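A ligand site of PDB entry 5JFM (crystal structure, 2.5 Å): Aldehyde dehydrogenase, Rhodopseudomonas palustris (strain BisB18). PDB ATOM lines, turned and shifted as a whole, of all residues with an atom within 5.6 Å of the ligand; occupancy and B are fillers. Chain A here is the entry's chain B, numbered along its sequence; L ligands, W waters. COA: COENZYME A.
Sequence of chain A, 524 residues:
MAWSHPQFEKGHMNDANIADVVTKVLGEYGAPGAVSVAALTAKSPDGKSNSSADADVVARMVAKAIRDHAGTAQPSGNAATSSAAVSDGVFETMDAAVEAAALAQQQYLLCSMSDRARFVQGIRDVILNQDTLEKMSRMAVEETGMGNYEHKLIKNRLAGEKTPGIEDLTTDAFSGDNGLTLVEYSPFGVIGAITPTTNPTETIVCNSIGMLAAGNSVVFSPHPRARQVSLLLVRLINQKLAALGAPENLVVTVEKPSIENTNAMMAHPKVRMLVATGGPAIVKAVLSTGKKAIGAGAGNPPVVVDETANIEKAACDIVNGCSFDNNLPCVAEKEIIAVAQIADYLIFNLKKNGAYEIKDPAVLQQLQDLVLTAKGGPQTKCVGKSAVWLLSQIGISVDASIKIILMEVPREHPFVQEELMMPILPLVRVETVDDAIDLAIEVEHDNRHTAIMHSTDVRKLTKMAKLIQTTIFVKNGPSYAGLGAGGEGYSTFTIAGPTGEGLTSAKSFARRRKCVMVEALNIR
Water W3 bridges N7A of the ligand and O of Thr 277.
The backbone carbonyl oxygen (O) of Pro 222 sits close to a nitrogen (N1A) of the ligand.
Merely in contact with the ligand: Ile 194 (3.2 Å), Pro 196 (3.5 Å), Thr 197 (3.5 Å), Thr 198 (3.3 Å), Ser 258 (3.5 Å), Ile 259 (3.3 Å), Thr 277 (3.7 Å), Gly 278 (3.6 Å), Gly 279 (3.4 Å), Ala 281 (3.7 Å), Ile 282 (3.8 Å) and Met 421 (3.9 Å).
Of the 30 residues printed, 21 come within 4 Å of the ligand.
OG1 of Thr 262 lies within hydrogen-bond range of O of Ser 258, 3.1 Å away.
O of Asn 199 is in hydrogen-bond range of OG1 of Thr 203 (2.9 Å).
O of Ile 194 is in hydrogen-bond range of N of Thr 277 (2.9 Å).
The side-chain hydroxyl of Thr 494 sits at hydrogen-bond distance from the side-chain hydroxyl of Thr 277, 2.8 Å away.
O5B of the ligand sits at hydrogen-bond distance from NE2 of His 223.
O of Ser 221 sits at hydrogen-bond distance from N6A of the ligand (2.9 Å).
N1A of the ligand is in hydrogen-bond range of OG1 of Thr 262, at 2.9 Å.
The side-chain amide nitrogen of Asn 199 lies close to a sulfur (S1P) of the ligand (3.0 Å).
The backbone carbonyl oxygen (O) of Thr 195 is in hydrogen-bond range of a nitrogen (N6A) of the ligand, 3.1 Å away.
O of Phe 493 lies close to S1P of the ligand, at 3.2 Å.
The side-chain sulfur (SG) of Cys 330 sits close to a sulfur (S1P) of the ligand (3.3 Å).
The side-chain hydroxyl (OG1) of Thr 380 lies within hydrogen-bond range of an oxygen (O5A) of the ligand (3.4 Å).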
ATOM      1  N   MET A 146      22.692  -3.291  -7.937  1.00  0.00           N
ATOM      2  CA  MET A 146      22.125  -2.827  -6.680  1.00  0.00           C
ATOM      3  C   MET A 146      22.762  -3.574  -5.528  1.00  0.00           C
ATOM      4  O   MET A 146      23.043  -4.768  -5.630  1.00  0.00           O
ATOM      5  CB  MET A 146      20.612  -3.034  -6.674  1.00  0.00           C
ATOM      6  CG  MET A 146      19.927  -2.440  -7.900  1.00  0.00           C
ATOM      7  SD  MET A 146      18.139  -2.605  -7.855  1.00  0.00           S
ATOM      8  CE  MET A 146      17.934  -4.386  -7.862  1.00  0.00           C
ATOM      9  N   ILE A 194       7.523 -16.153  -5.911  1.00  0.00           N
ATOM     10  CA  ILE A 194       8.003 -15.021  -6.695  1.00  0.00           C
ATOM     11  C   ILE A 194       9.040 -14.282  -5.862  1.00  0.00           C
ATOM     12  O   ILE A 194       8.726 -13.784  -4.775  1.00  0.00           O
ATOM     13  CB  ILE A 194       6.846 -14.106  -7.100  1.00  0.00           C
ATOM     14  CG1 ILE A 194       5.807 -14.892  -7.887  1.00  0.00           C
ATOM     15  CG2 ILE A 194       7.338 -12.914  -7.891  1.00  0.00           C
ATOM     16  CD1 ILE A 194       4.492 -14.192  -8.056  1.00  0.00           C
ATOM     17  N   THR A 195      10.246 -14.219  -6.347  1.00  0.00           N
ATOM     18  CA  THR A 195      11.332 -13.638  -5.576  1.00  0.00           C
ATOM     19  C   THR A 195      11.780 -12.318  -6.188  1.00  0.00           C
ATOM     20  O   THR A 195      11.600 -12.100  -7.385  1.00  0.00           O
ATOM     21  CB  THR A 195      12.503 -14.617  -5.474  1.00  0.00           C
ATOM     22  OG1 THR A 195      12.976 -14.933  -6.793  1.00  0.00           O
ATOM     23  CG2 THR A 195      12.044 -15.898  -4.804  1.00  0.00           C
ATOM     24  N   PRO A 196      12.336 -11.404  -5.394  1.00  0.00           N
ATOM     25  CA  PRO A 196      12.611 -10.051  -5.896  1.00  0.00           C
ATOM     26  C   PRO A 196      14.021  -9.911  -6.442  1.00  0.00           C
ATOM     27  O   PRO A 196      14.929 -10.702  -6.171  1.00  0.00           O
ATOM     28  CB  PRO A 196      12.441  -9.193  -4.636  1.00  0.00           C
ATOM     29  CG  PRO A 196      12.984 -10.084  -3.558  1.00  0.00           C
ATOM     30  CD  PRO A 196      12.597 -11.504  -3.944  1.00  0.00           C
ATOM     31  N   THR A 197      14.207  -8.843  -7.215  1.00  0.00           N
ATOM     32  CA  THR A 197      15.534  -8.504  -7.690  1.00  0.00           C
ATOM     33  C   THR A 197      16.385  -7.862  -6.604  1.00  0.00           C
ATOM     34  O   THR A 197      17.607  -7.791  -6.754  1.00  0.00           O
ATOM     35  CB  THR A 197      15.427  -7.579  -8.884  1.00  0.00           C
ATOM     36  OG1 THR A 197      16.748  -7.256  -9.363  1.00  0.00           O
ATOM     37  CG2 THR A 197      14.716  -6.313  -8.495  1.00  0.00           C
ATOM     38  N   THR A 198      15.757  -7.434  -5.504  1.00  0.00           N
ATOM     39  CA  THR A 198      16.504  -6.827  -4.412  1.00  0.00           C
ATOM     40  C   THR A 198      17.322  -7.870  -3.643  1.00  0.00           C
ATOM     41  O   THR A 198      18.519  -7.690  -3.423  1.00  0.00           O
ATOM     42  CB  THR A 198      15.531  -6.085  -3.497  1.00  0.00           C
ATOM     43  OG1 THR A 198      15.250  -4.812  -4.042  1.00  0.00           O
ATOM     44  CG2 THR A 198      16.076  -5.937  -2.106  1.00  0.00           C
ATOM     45  N   ASN A 199      16.683  -8.967  -3.242  1.00  0.00           N
ATOM     46  CA  ASN A 199      17.356 -10.020  -2.484  1.00  0.00           C
ATOM     47  C   ASN A 199      17.165 -11.355  -3.195  1.00  0.00           C
ATOM     48  O   ASN A 199      16.529 -12.281  -2.677  1.00  0.00           O
ATOM     49  CB  ASN A 199      16.823 -10.081  -1.050  1.00  0.00           C
ATOM     50  CG  ASN A 199      17.046  -8.773  -0.299  1.00  0.00           C
ATOM     51  OD1 ASN A 199      18.116  -8.162  -0.387  1.00  0.00           O
ATOM     52  ND2 ASN A 199      16.027  -8.335   0.438  1.00  0.00           N
ATOM     53  N   THR A 203      16.234 -14.627  -0.624  1.00  0.00           N
ATOM     54  CA  THR A 203      14.859 -15.104  -0.681  1.00  0.00           C
ATOM     55  C   THR A 203      14.778 -16.542  -1.172  1.00  0.00           C
ATOM     56  O   THR A 203      13.956 -17.322  -0.657  1.00  0.00           O
ATOM     57  CB  THR A 203      14.039 -14.171  -1.564  1.00  0.00           C
ATOM     58  OG1 THR A 203      14.165 -12.835  -1.073  1.00  0.00           O
ATOM     59  CG2 THR A 203      12.566 -14.556  -1.520  1.00  0.00           C
ATOM     60  N   SER A 221       9.704 -18.285  -9.808  1.00  0.00           N
ATOM     61  CA  SER A 221       9.692 -17.309 -10.883  1.00  0.00           C
ATOM     62  C   SER A 221      10.528 -16.121 -10.432  1.00  0.00           C
ATOM     63  O   SER A 221      10.003 -15.187  -9.810  1.00  0.00           O
ATOM     64  CB  SER A 221       8.267 -16.848 -11.224  1.00  0.00           C
ATOM     65  OG  SER A 221       7.547 -17.849 -11.891  1.00  0.00           O
ATOM     66  N   PRO A 222      11.828 -16.109 -10.678  1.00  0.00           N
ATOM     67  CA  PRO A 222      12.652 -14.982 -10.243  1.00  0.00           C
ATOM     68  C   PRO A 222      12.492 -13.789 -11.172  1.00  0.00           C
ATOM     69  O   PRO A 222      11.867 -13.862 -12.238  1.00  0.00           O
ATOM     70  CB  PRO A 222      14.069 -15.547 -10.288  1.00  0.00           C
ATOM     71  CG  PRO A 222      14.012 -16.525 -11.400  1.00  0.00           C
ATOM     72  CD  PRO A 222      12.631 -17.154 -11.337  1.00  0.00           C
ATOM     73  N   HIS A 223      13.044 -12.668 -10.741  1.00  0.00           N
ATOM     74  CA  HIS A 223      13.004 -11.467 -11.560  1.00  0.00           C
ATOM     75  C   HIS A 223      14.004 -11.594 -12.703  1.00  0.00           C
ATOM     76  O   HIS A 223      15.105 -12.120 -12.510  1.00  0.00           O
ATOM     77  CB  HIS A 223      13.324 -10.244 -10.700  1.00  0.00           C
ATOM     78  CG  HIS A 223      12.562  -9.020 -11.104  1.00  0.00           C
ATOM     79  ND1 HIS A 223      12.947  -8.223 -12.158  1.00  0.00           N
ATOM     80  CD2 HIS A 223      11.436  -8.459 -10.598  1.00  0.00           C
ATOM     81  CE1 HIS A 223      12.084  -7.223 -12.293  1.00  0.00           C
ATOM     82  NE2 HIS A 223      11.164  -7.344 -11.354  1.00  0.00           N
ATOM     83  N   PRO A 224      13.643 -11.148 -13.910  1.00  0.00           N
ATOM     84  CA  PRO A 224      14.603 -11.212 -15.020  1.00  0.00           C
ATOM     85  C   PRO A 224      15.902 -10.467 -14.746  1.00  0.00           C
ATOM     86  O   PRO A 224      16.969 -10.906 -15.208  1.00  0.00           O
ATOM     87  CB  PRO A 224      13.837 -10.589 -16.203  1.00  0.00           C
ATOM     88  CG  PRO A 224      12.419 -10.502 -15.783  1.00  0.00           C
ATOM     89  CD  PRO A 224      12.263 -10.905 -14.351  1.00  0.00           C
ATOM     90  N   ARG A 225      15.861  -9.378 -13.982  1.00  0.00           N
ATOM     91  CA  ARG A 225      17.080  -8.640 -13.668  1.00  0.00           C
ATOM     92  C   ARG A 225      18.054  -9.438 -12.814  1.00  0.00           C
ATOM     93  O   ARG A 225      19.195  -9.004 -12.659  1.00  0.00           O
ATOM     94  CB  ARG A 225      16.731  -7.332 -12.957  1.00  0.00           C
ATOM     95  CG  ARG A 225      15.973  -6.326 -13.813  1.00  0.00           C
ATOM     96  CD  ARG A 225      16.747  -5.978 -15.094  1.00  0.00           C
ATOM     97  NE  ARG A 225      15.852  -5.489 -16.155  1.00  0.00           N
ATOM     98  CZ  ARG A 225      16.254  -4.952 -17.303  1.00  0.00           C
ATOM     99  NH1 ARG A 225      17.543  -4.812 -17.569  1.00  0.00           N
ATOM    100  NH2 ARG A 225      15.346  -4.551 -18.186  1.00  0.00           N
ATOM    101  N   SER A 258      10.172 -14.442 -16.751  1.00  0.00           N
ATOM    102  CA  SER A 258       9.420 -13.352 -17.368  1.00  0.00           C
ATOM    103  C   SER A 258       8.152 -13.109 -16.560  1.00  0.00           C
ATOM    104  O   SER A 258       7.725 -13.949 -15.758  1.00  0.00           O
ATOM    105  CB  SER A 258       9.052 -13.664 -18.825  1.00  0.00           C
ATOM    106  OG  SER A 258       8.053 -14.676 -18.888  1.00  0.00           O
ATOM    107  N   ILE A 259       7.527 -11.956 -16.813  1.00  0.00           N
ATOM    108  CA  ILE A 259       6.196 -11.754 -16.238  1.00  0.00           C
ATOM    109  C   ILE A 259       5.194 -12.697 -16.898  1.00  0.00           C
ATOM    110  O   ILE A 259       4.206 -13.111 -16.259  1.00  0.00           O
ATOM    111  CB  ILE A 259       5.778 -10.277 -16.338  1.00  0.00           C
ATOM    112  CG1 ILE A 259       4.512 -10.038 -15.517  1.00  0.00           C
ATOM    113  CG2 ILE A 259       5.532  -9.866 -17.774  1.00  0.00           C
ATOM    114  CD1 ILE A 259       4.557 -10.676 -14.125  1.00  0.00           C
ATOM    115  N   THR A 262       5.586 -15.951 -14.887  1.00  0.00           N
ATOM    116  CA  THR A 262       5.035 -15.750 -13.554  1.00  0.00           C
ATOM    117  C   THR A 262       3.511 -15.862 -13.563  1.00  0.00           C
ATOM    118  O   THR A 262       2.923 -16.524 -12.699  1.00  0.00           O
ATOM    119  CB  THR A 262       5.452 -14.394 -13.019  1.00  0.00           C
ATOM    120  OG1 THR A 262       6.877 -14.399 -12.827  1.00  0.00           O
ATOM    121  CG2 THR A 262       4.757 -14.109 -11.698  1.00  0.00           C
ATOM    122  N   THR A 277       7.221 -12.193  -2.904  1.00  0.00           N
ATOM    123  CA  THR A 277       8.068 -11.226  -2.229  1.00  0.00           C
ATOM    124  C   THR A 277       8.408 -10.157  -3.256  1.00  0.00           C
ATOM    125  O   THR A 277       9.224 -10.385  -4.154  1.00  0.00           O
ATOM    126  CB  THR A 277       9.310 -11.891  -1.659  1.00  0.00           C
ATOM    127  OG1 THR A 277       8.928 -12.914  -0.739  1.00  0.00           O
ATOM    128  CG2 THR A 277      10.181 -10.864  -0.955  1.00  0.00           C
ATOM    129  N   GLY A 278       7.771  -9.001  -3.140  1.00  0.00           N
ATOM    130  CA  GLY A 278       7.969  -7.940  -4.111  1.00  0.00           C
ATOM    131  C   GLY A 278       7.136  -6.728  -3.764  1.00  0.00           C
ATOM    132  O   GLY A 278       6.755  -6.529  -2.612  1.00  0.00           O
ATOM    133  N   GLY A 279       6.854  -5.916  -4.786  1.00  0.00           N
ATOM    134  CA  GLY A 279       6.059  -4.721  -4.628  1.00  0.00           C
ATOM    135  C   GLY A 279       4.578  -5.021  -4.595  1.00  0.00           C
ATOM    136  O   GLY A 279       4.118  -6.158  -4.806  1.00  0.00           O
ATOM    137  N   ALA A 281       2.101  -4.392  -6.551  1.00  0.00           N
ATOM    138  CA  ALA A 281       1.453  -4.902  -7.748  1.00  0.00           C
ATOM    139  C   ALA A 281       1.458  -6.426  -7.771  1.00  0.00           C
ATOM    140  O   ALA A 281       0.415  -7.067  -7.956  1.00  0.00           O
ATOM    141  CB  ALA A 281       2.138  -4.342  -8.999  1.00  0.00           C
ATOM    142  N   ILE A 282       2.630  -7.037  -7.562  1.00  0.00           N
ATOM    143  CA  ILE A 282       2.702  -8.487  -7.647  1.00  0.00           C
ATOM    144  C   ILE A 282       2.029  -9.123  -6.436  1.00  0.00           C
ATOM    145  O   ILE A 282       1.520 -10.252  -6.533  1.00  0.00           O
ATOM    146  CB  ILE A 282       4.167  -8.934  -7.815  1.00  0.00           C
ATOM    147  CG1 ILE A 282       4.255 -10.396  -8.241  1.00  0.00           C
ATOM    148  CG2 ILE A 282       4.949  -8.718  -6.523  1.00  0.00           C
ATOM    149  CD1 ILE A 282       3.554 -10.693  -9.540  1.00  0.00           C
ATOM    150  N   GLY A 297       4.755  -7.634   1.881  1.00  0.00           N
ATOM    151  CA  GLY A 297       4.601  -6.227   1.564  1.00  0.00           C
ATOM    152  C   GLY A 297       5.868  -5.399   1.748  1.00  0.00           C
ATOM    153  O   GLY A 297       6.971  -5.900   1.939  1.00  0.00           O
ATOM    154  N   ALA A 298       5.663  -4.083   1.673  1.00  0.00           N
ATOM    155  CA  ALA A 298       6.743  -3.096   1.723  1.00  0.00           C
ATOM    156  C   ALA A 298       6.314  -1.931   2.598  1.00  0.00           C
ATOM    157  O   ALA A 298       5.203  -1.920   3.158  1.00  0.00           O
ATOM    158  CB  ALA A 298       7.108  -2.619   0.310  1.00  0.00           C
ATOM    159  N   LEU A 328      18.730  -1.249   0.352  1.00  0.00           N
ATOM    160  CA  LEU A 328      17.832  -2.242  -0.249  1.00  0.00           C
ATOM    161  C   LEU A 328      16.881  -2.900   0.753  1.00  0.00           C
ATOM    162  O   LEU A 328      15.668  -2.873   0.506  1.00  0.00           O
ATOM    163  CB  LEU A 328      18.668  -3.277  -0.999  1.00  0.00           C
ATOM    164  CG  LEU A 328      18.893  -3.030  -2.503  1.00  0.00           C
ATOM    165  CD1 LEU A 328      19.361  -1.640  -2.733  1.00  0.00           C
ATOM    166  CD2 LEU A 328      19.907  -4.034  -3.092  1.00  0.00           C
ATOM    167  N   CYS A 330      14.275  -4.912   3.218  1.00  0.00           N
ATOM    168  CA  CYS A 330      12.872  -4.637   3.489  1.00  0.00           C
ATOM    169  C   CYS A 330      12.662  -3.788   4.738  1.00  0.00           C
ATOM    170  O   CYS A 330      11.596  -3.177   4.900  1.00  0.00           O
ATOM    171  CB  CYS A 330      12.141  -5.984   3.601  1.00  0.00           C
ATOM    172  SG  CYS A 330      13.256  -7.431   3.358  1.00  0.00           S
ATOM    173  N   THR A 380      15.553   4.284 -10.948  1.00  0.00           N
ATOM    174  CA  THR A 380      16.064   2.918 -10.793  1.00  0.00           C
ATOM    175  C   THR A 380      17.557   2.853 -11.046  1.00  0.00           C
ATOM    176  O   THR A 380      18.263   2.025 -10.465  1.00  0.00           O
ATOM    177  CB  THR A 380      15.293   1.965 -11.714  1.00  0.00           C
ATOM    178  OG1 THR A 380      13.875   2.145 -11.498  1.00  0.00           O
ATOM    179  CG2 THR A 380      15.650   0.512 -11.419  1.00  0.00           C
ATOM    180  N   VAL A 383      18.885   3.129  -7.534  1.00  0.00           N
ATOM    181  CA  VAL A 383      18.407   2.264  -6.456  1.00  0.00           C
ATOM    182  C   VAL A 383      19.543   1.356  -6.001  1.00  0.00           C
ATOM    183  O   VAL A 383      20.139   0.628  -6.796  1.00  0.00           O
ATOM    184  CB  VAL A 383      17.194   1.456  -6.903  1.00  0.00           C
ATOM    185  CG1 VAL A 383      16.993   0.267  -5.969  1.00  0.00           C
ATOM    186  CG2 VAL A 383      15.959   2.349  -6.945  1.00  0.00           C
ATOM    187  N   MET A 421      14.949   3.510  -1.388  1.00  0.00           N
ATOM    188  CA  MET A 421      15.871   2.382  -1.330  1.00  0.00           C
ATOM    189  C   MET A 421      17.274   2.822  -1.757  1.00  0.00           C
ATOM    190  O   MET A 421      17.914   2.235  -2.629  1.00  0.00           O
ATOM    191  CB  MET A 421      15.370   1.198  -2.174  1.00  0.00           C
ATOM    192  CG  MET A 421      13.851   1.065  -2.227  1.00  0.00           C
ATOM    193  SD  MET A 421      13.283  -0.303  -3.279  1.00  0.00           S
ATOM    194  CE  MET A 421      13.771  -1.711  -2.261  1.00  0.00           C
ATOM    195  N   PHE A 493      13.372 -13.584   4.688  1.00  0.00           N
ATOM    196  CA  PHE A 493      13.360 -12.493   3.714  1.00  0.00           C
ATOM    197  C   PHE A 493      12.024 -12.430   2.997  1.00  0.00           C
ATOM    198  O   PHE A 493      11.907 -11.771   1.957  1.00  0.00           O
ATOM    199  CB  PHE A 493      14.524 -12.640   2.734  1.00  0.00           C
ATOM    200  CG  PHE A 493      15.835 -12.322   3.358  1.00  0.00           C
ATOM    201  CD1 PHE A 493      16.549 -13.291   4.023  1.00  0.00           C
ATOM    202  CD2 PHE A 493      16.323 -11.021   3.344  1.00  0.00           C
ATOM    203  CE1 PHE A 493      17.741 -12.997   4.635  1.00  0.00           C
ATOM    204  CE2 PHE A 493      17.525 -10.724   3.956  1.00  0.00           C
ATOM    205  CZ  PHE A 493      18.236 -11.719   4.599  1.00  0.00           C
ATOM    206  N   THR A 494      11.017 -13.092   3.545  1.00  0.00           N
ATOM    207  CA  THR A 494       9.631 -12.954   3.133  1.00  0.00           C
ATOM    208  C   THR A 494       8.868 -12.536   4.392  1.00  0.00           C
ATOM    209  O   THR A 494       8.525 -13.367   5.243  1.00  0.00           O
ATOM    210  CB  THR A 494       9.134 -14.243   2.489  1.00  0.00           C
ATOM    211  OG1 THR A 494       9.943 -14.527   1.337  1.00  0.00           O
ATOM    212  CG2 THR A 494       7.682 -14.136   2.041  1.00  0.00           C
HETATM  213  N1A COA L   1       8.750 -12.279 -12.090  1.00  0.00           N
HETATM  214  C2A COA L   1       8.039 -11.664 -13.082  1.00  0.00           C
HETATM  215  N3A COA L   1       7.570 -10.395 -12.892  1.00  0.00           N
HETATM  216  C4A COA L   1       7.806  -9.729 -11.728  1.00  0.00           C
HETATM  217  C5A COA L   1       8.514 -10.340 -10.749  1.00  0.00           C
HETATM  218  C6A COA L   1       8.987 -11.618 -10.934  1.00  0.00           C
HETATM  219  N6A COA L   1       9.758 -12.312  -9.907  1.00  0.00           N
HETATM  220  N7A COA L   1       8.613  -9.466  -9.682  1.00  0.00           N
HETATM  221  C8A COA L   1       7.964  -8.317 -10.013  1.00  0.00           C
HETATM  222  N9A COA L   1       7.458  -8.470 -11.284  1.00  0.00           N
HETATM  223  C1B COA L   1       6.708  -7.574 -12.085  1.00  0.00           C
HETATM  224  C2B COA L   1       5.962  -6.778 -11.306  1.00  0.00           C
HETATM  225  O2B COA L   1       4.590  -7.295 -11.174  1.00  0.00           O
HETATM  226  C3B COA L   1       5.990  -5.442 -12.006  1.00  0.00           C
HETATM  227  O3B COA L   1       5.076  -5.398 -13.016  1.00  0.00           O
HETATM  228  P3B COA L   1       4.439  -3.976 -13.404  1.00  0.00           P
HETATM  229  O7A COA L   1       3.216  -3.732 -12.536  1.00  0.00           O
HETATM  230  O8A COA L   1       5.459  -2.872 -13.183  1.00  0.00           O
HETATM  231  O9A COA L   1       4.020  -4.008 -14.861  1.00  0.00           O
HETATM  232  C4B COA L   1       7.424  -5.384 -12.609  1.00  0.00           C
HETATM  233  O4B COA L   1       7.724  -6.634 -12.894  1.00  0.00           O
HETATM  234  C5B COA L   1       8.397  -4.806 -11.590  1.00  0.00           C
HETATM  235  O5B COA L   1       9.728  -5.082 -12.037  1.00  0.00           O
HETATM  236  P1A COA L   1      10.666  -3.878 -12.505  1.00  0.00           P
HETATM  237  O1A COA L   1       9.904  -2.973 -13.457  1.00  0.00           O
HETATM  238  O2A COA L   1      11.885  -4.438 -13.227  1.00  0.00           O
HETATM  239  O3A COA L   1      11.133  -3.026 -11.195  1.00  0.00           O
HETATM  240  P2A COA L   1      12.494  -2.144 -11.084  1.00  0.00           P
HETATM  241  O4A COA L   1      13.286  -2.176 -12.375  1.00  0.00           O
HETATM  242  O5A COA L   1      12.134  -0.701 -10.734  1.00  0.00           O
HETATM  243  O6A COA L   1      13.391  -2.776  -9.872  1.00  0.00           O
HETATM  244  CBP COA L   1      12.859  -2.547  -7.482  1.00  0.00           C
HETATM  245  CCP COA L   1      12.719  -3.437  -8.816  1.00  0.00           C
HETATM  246  CDP COA L   1      13.499  -3.377  -6.378  1.00  0.00           C
HETATM  247  CEP COA L   1      13.735  -1.347  -7.763  1.00  0.00           C
HETATM  248  CAP COA L   1      11.481  -2.065  -7.042  1.00  0.00           C
HETATM  249  OAP COA L   1      10.778  -1.617  -8.130  1.00  0.00           O
HETATM  250  C9P COA L   1      10.670  -3.207  -6.390  1.00  0.00           C
HETATM  251  O9P COA L   1      10.096  -4.014  -7.082  1.00  0.00           O
HETATM  252  N8P COA L   1      10.605  -3.279  -4.956  1.00  0.00           N
HETATM  253  C7P COA L   1       9.857  -4.353  -4.286  1.00  0.00           C
HETATM  254  C6P COA L   1      10.787  -5.553  -4.146  1.00  0.00           C
HETATM  255  C5P COA L   1      11.144  -5.782  -2.688  1.00  0.00           C
HETATM  256  O5P COA L   1      11.388  -4.834  -1.979  1.00  0.00           O
HETATM  257  N4P COA L   1      11.193  -7.117  -2.126  1.00  0.00           N
HETATM  258  C3P COA L   1      11.543  -7.307  -0.746  1.00  0.00           C
HETATM  259  C2P COA L   1      12.998  -7.839  -0.669  1.00  0.00           C
HETATM  260  S1P COA L   1      13.130  -9.161   0.525  1.00  0.00           S
HETATM  261  O   HOH W   1       8.773  -8.852 -14.917  1.00  0.00           O
HETATM  262  O   HOH W   2       8.923  -5.674  -8.604  1.00  0.00           O
HETATM  263  O   HOH W   3       9.317  -9.322  -6.991  1.00  0.00           O
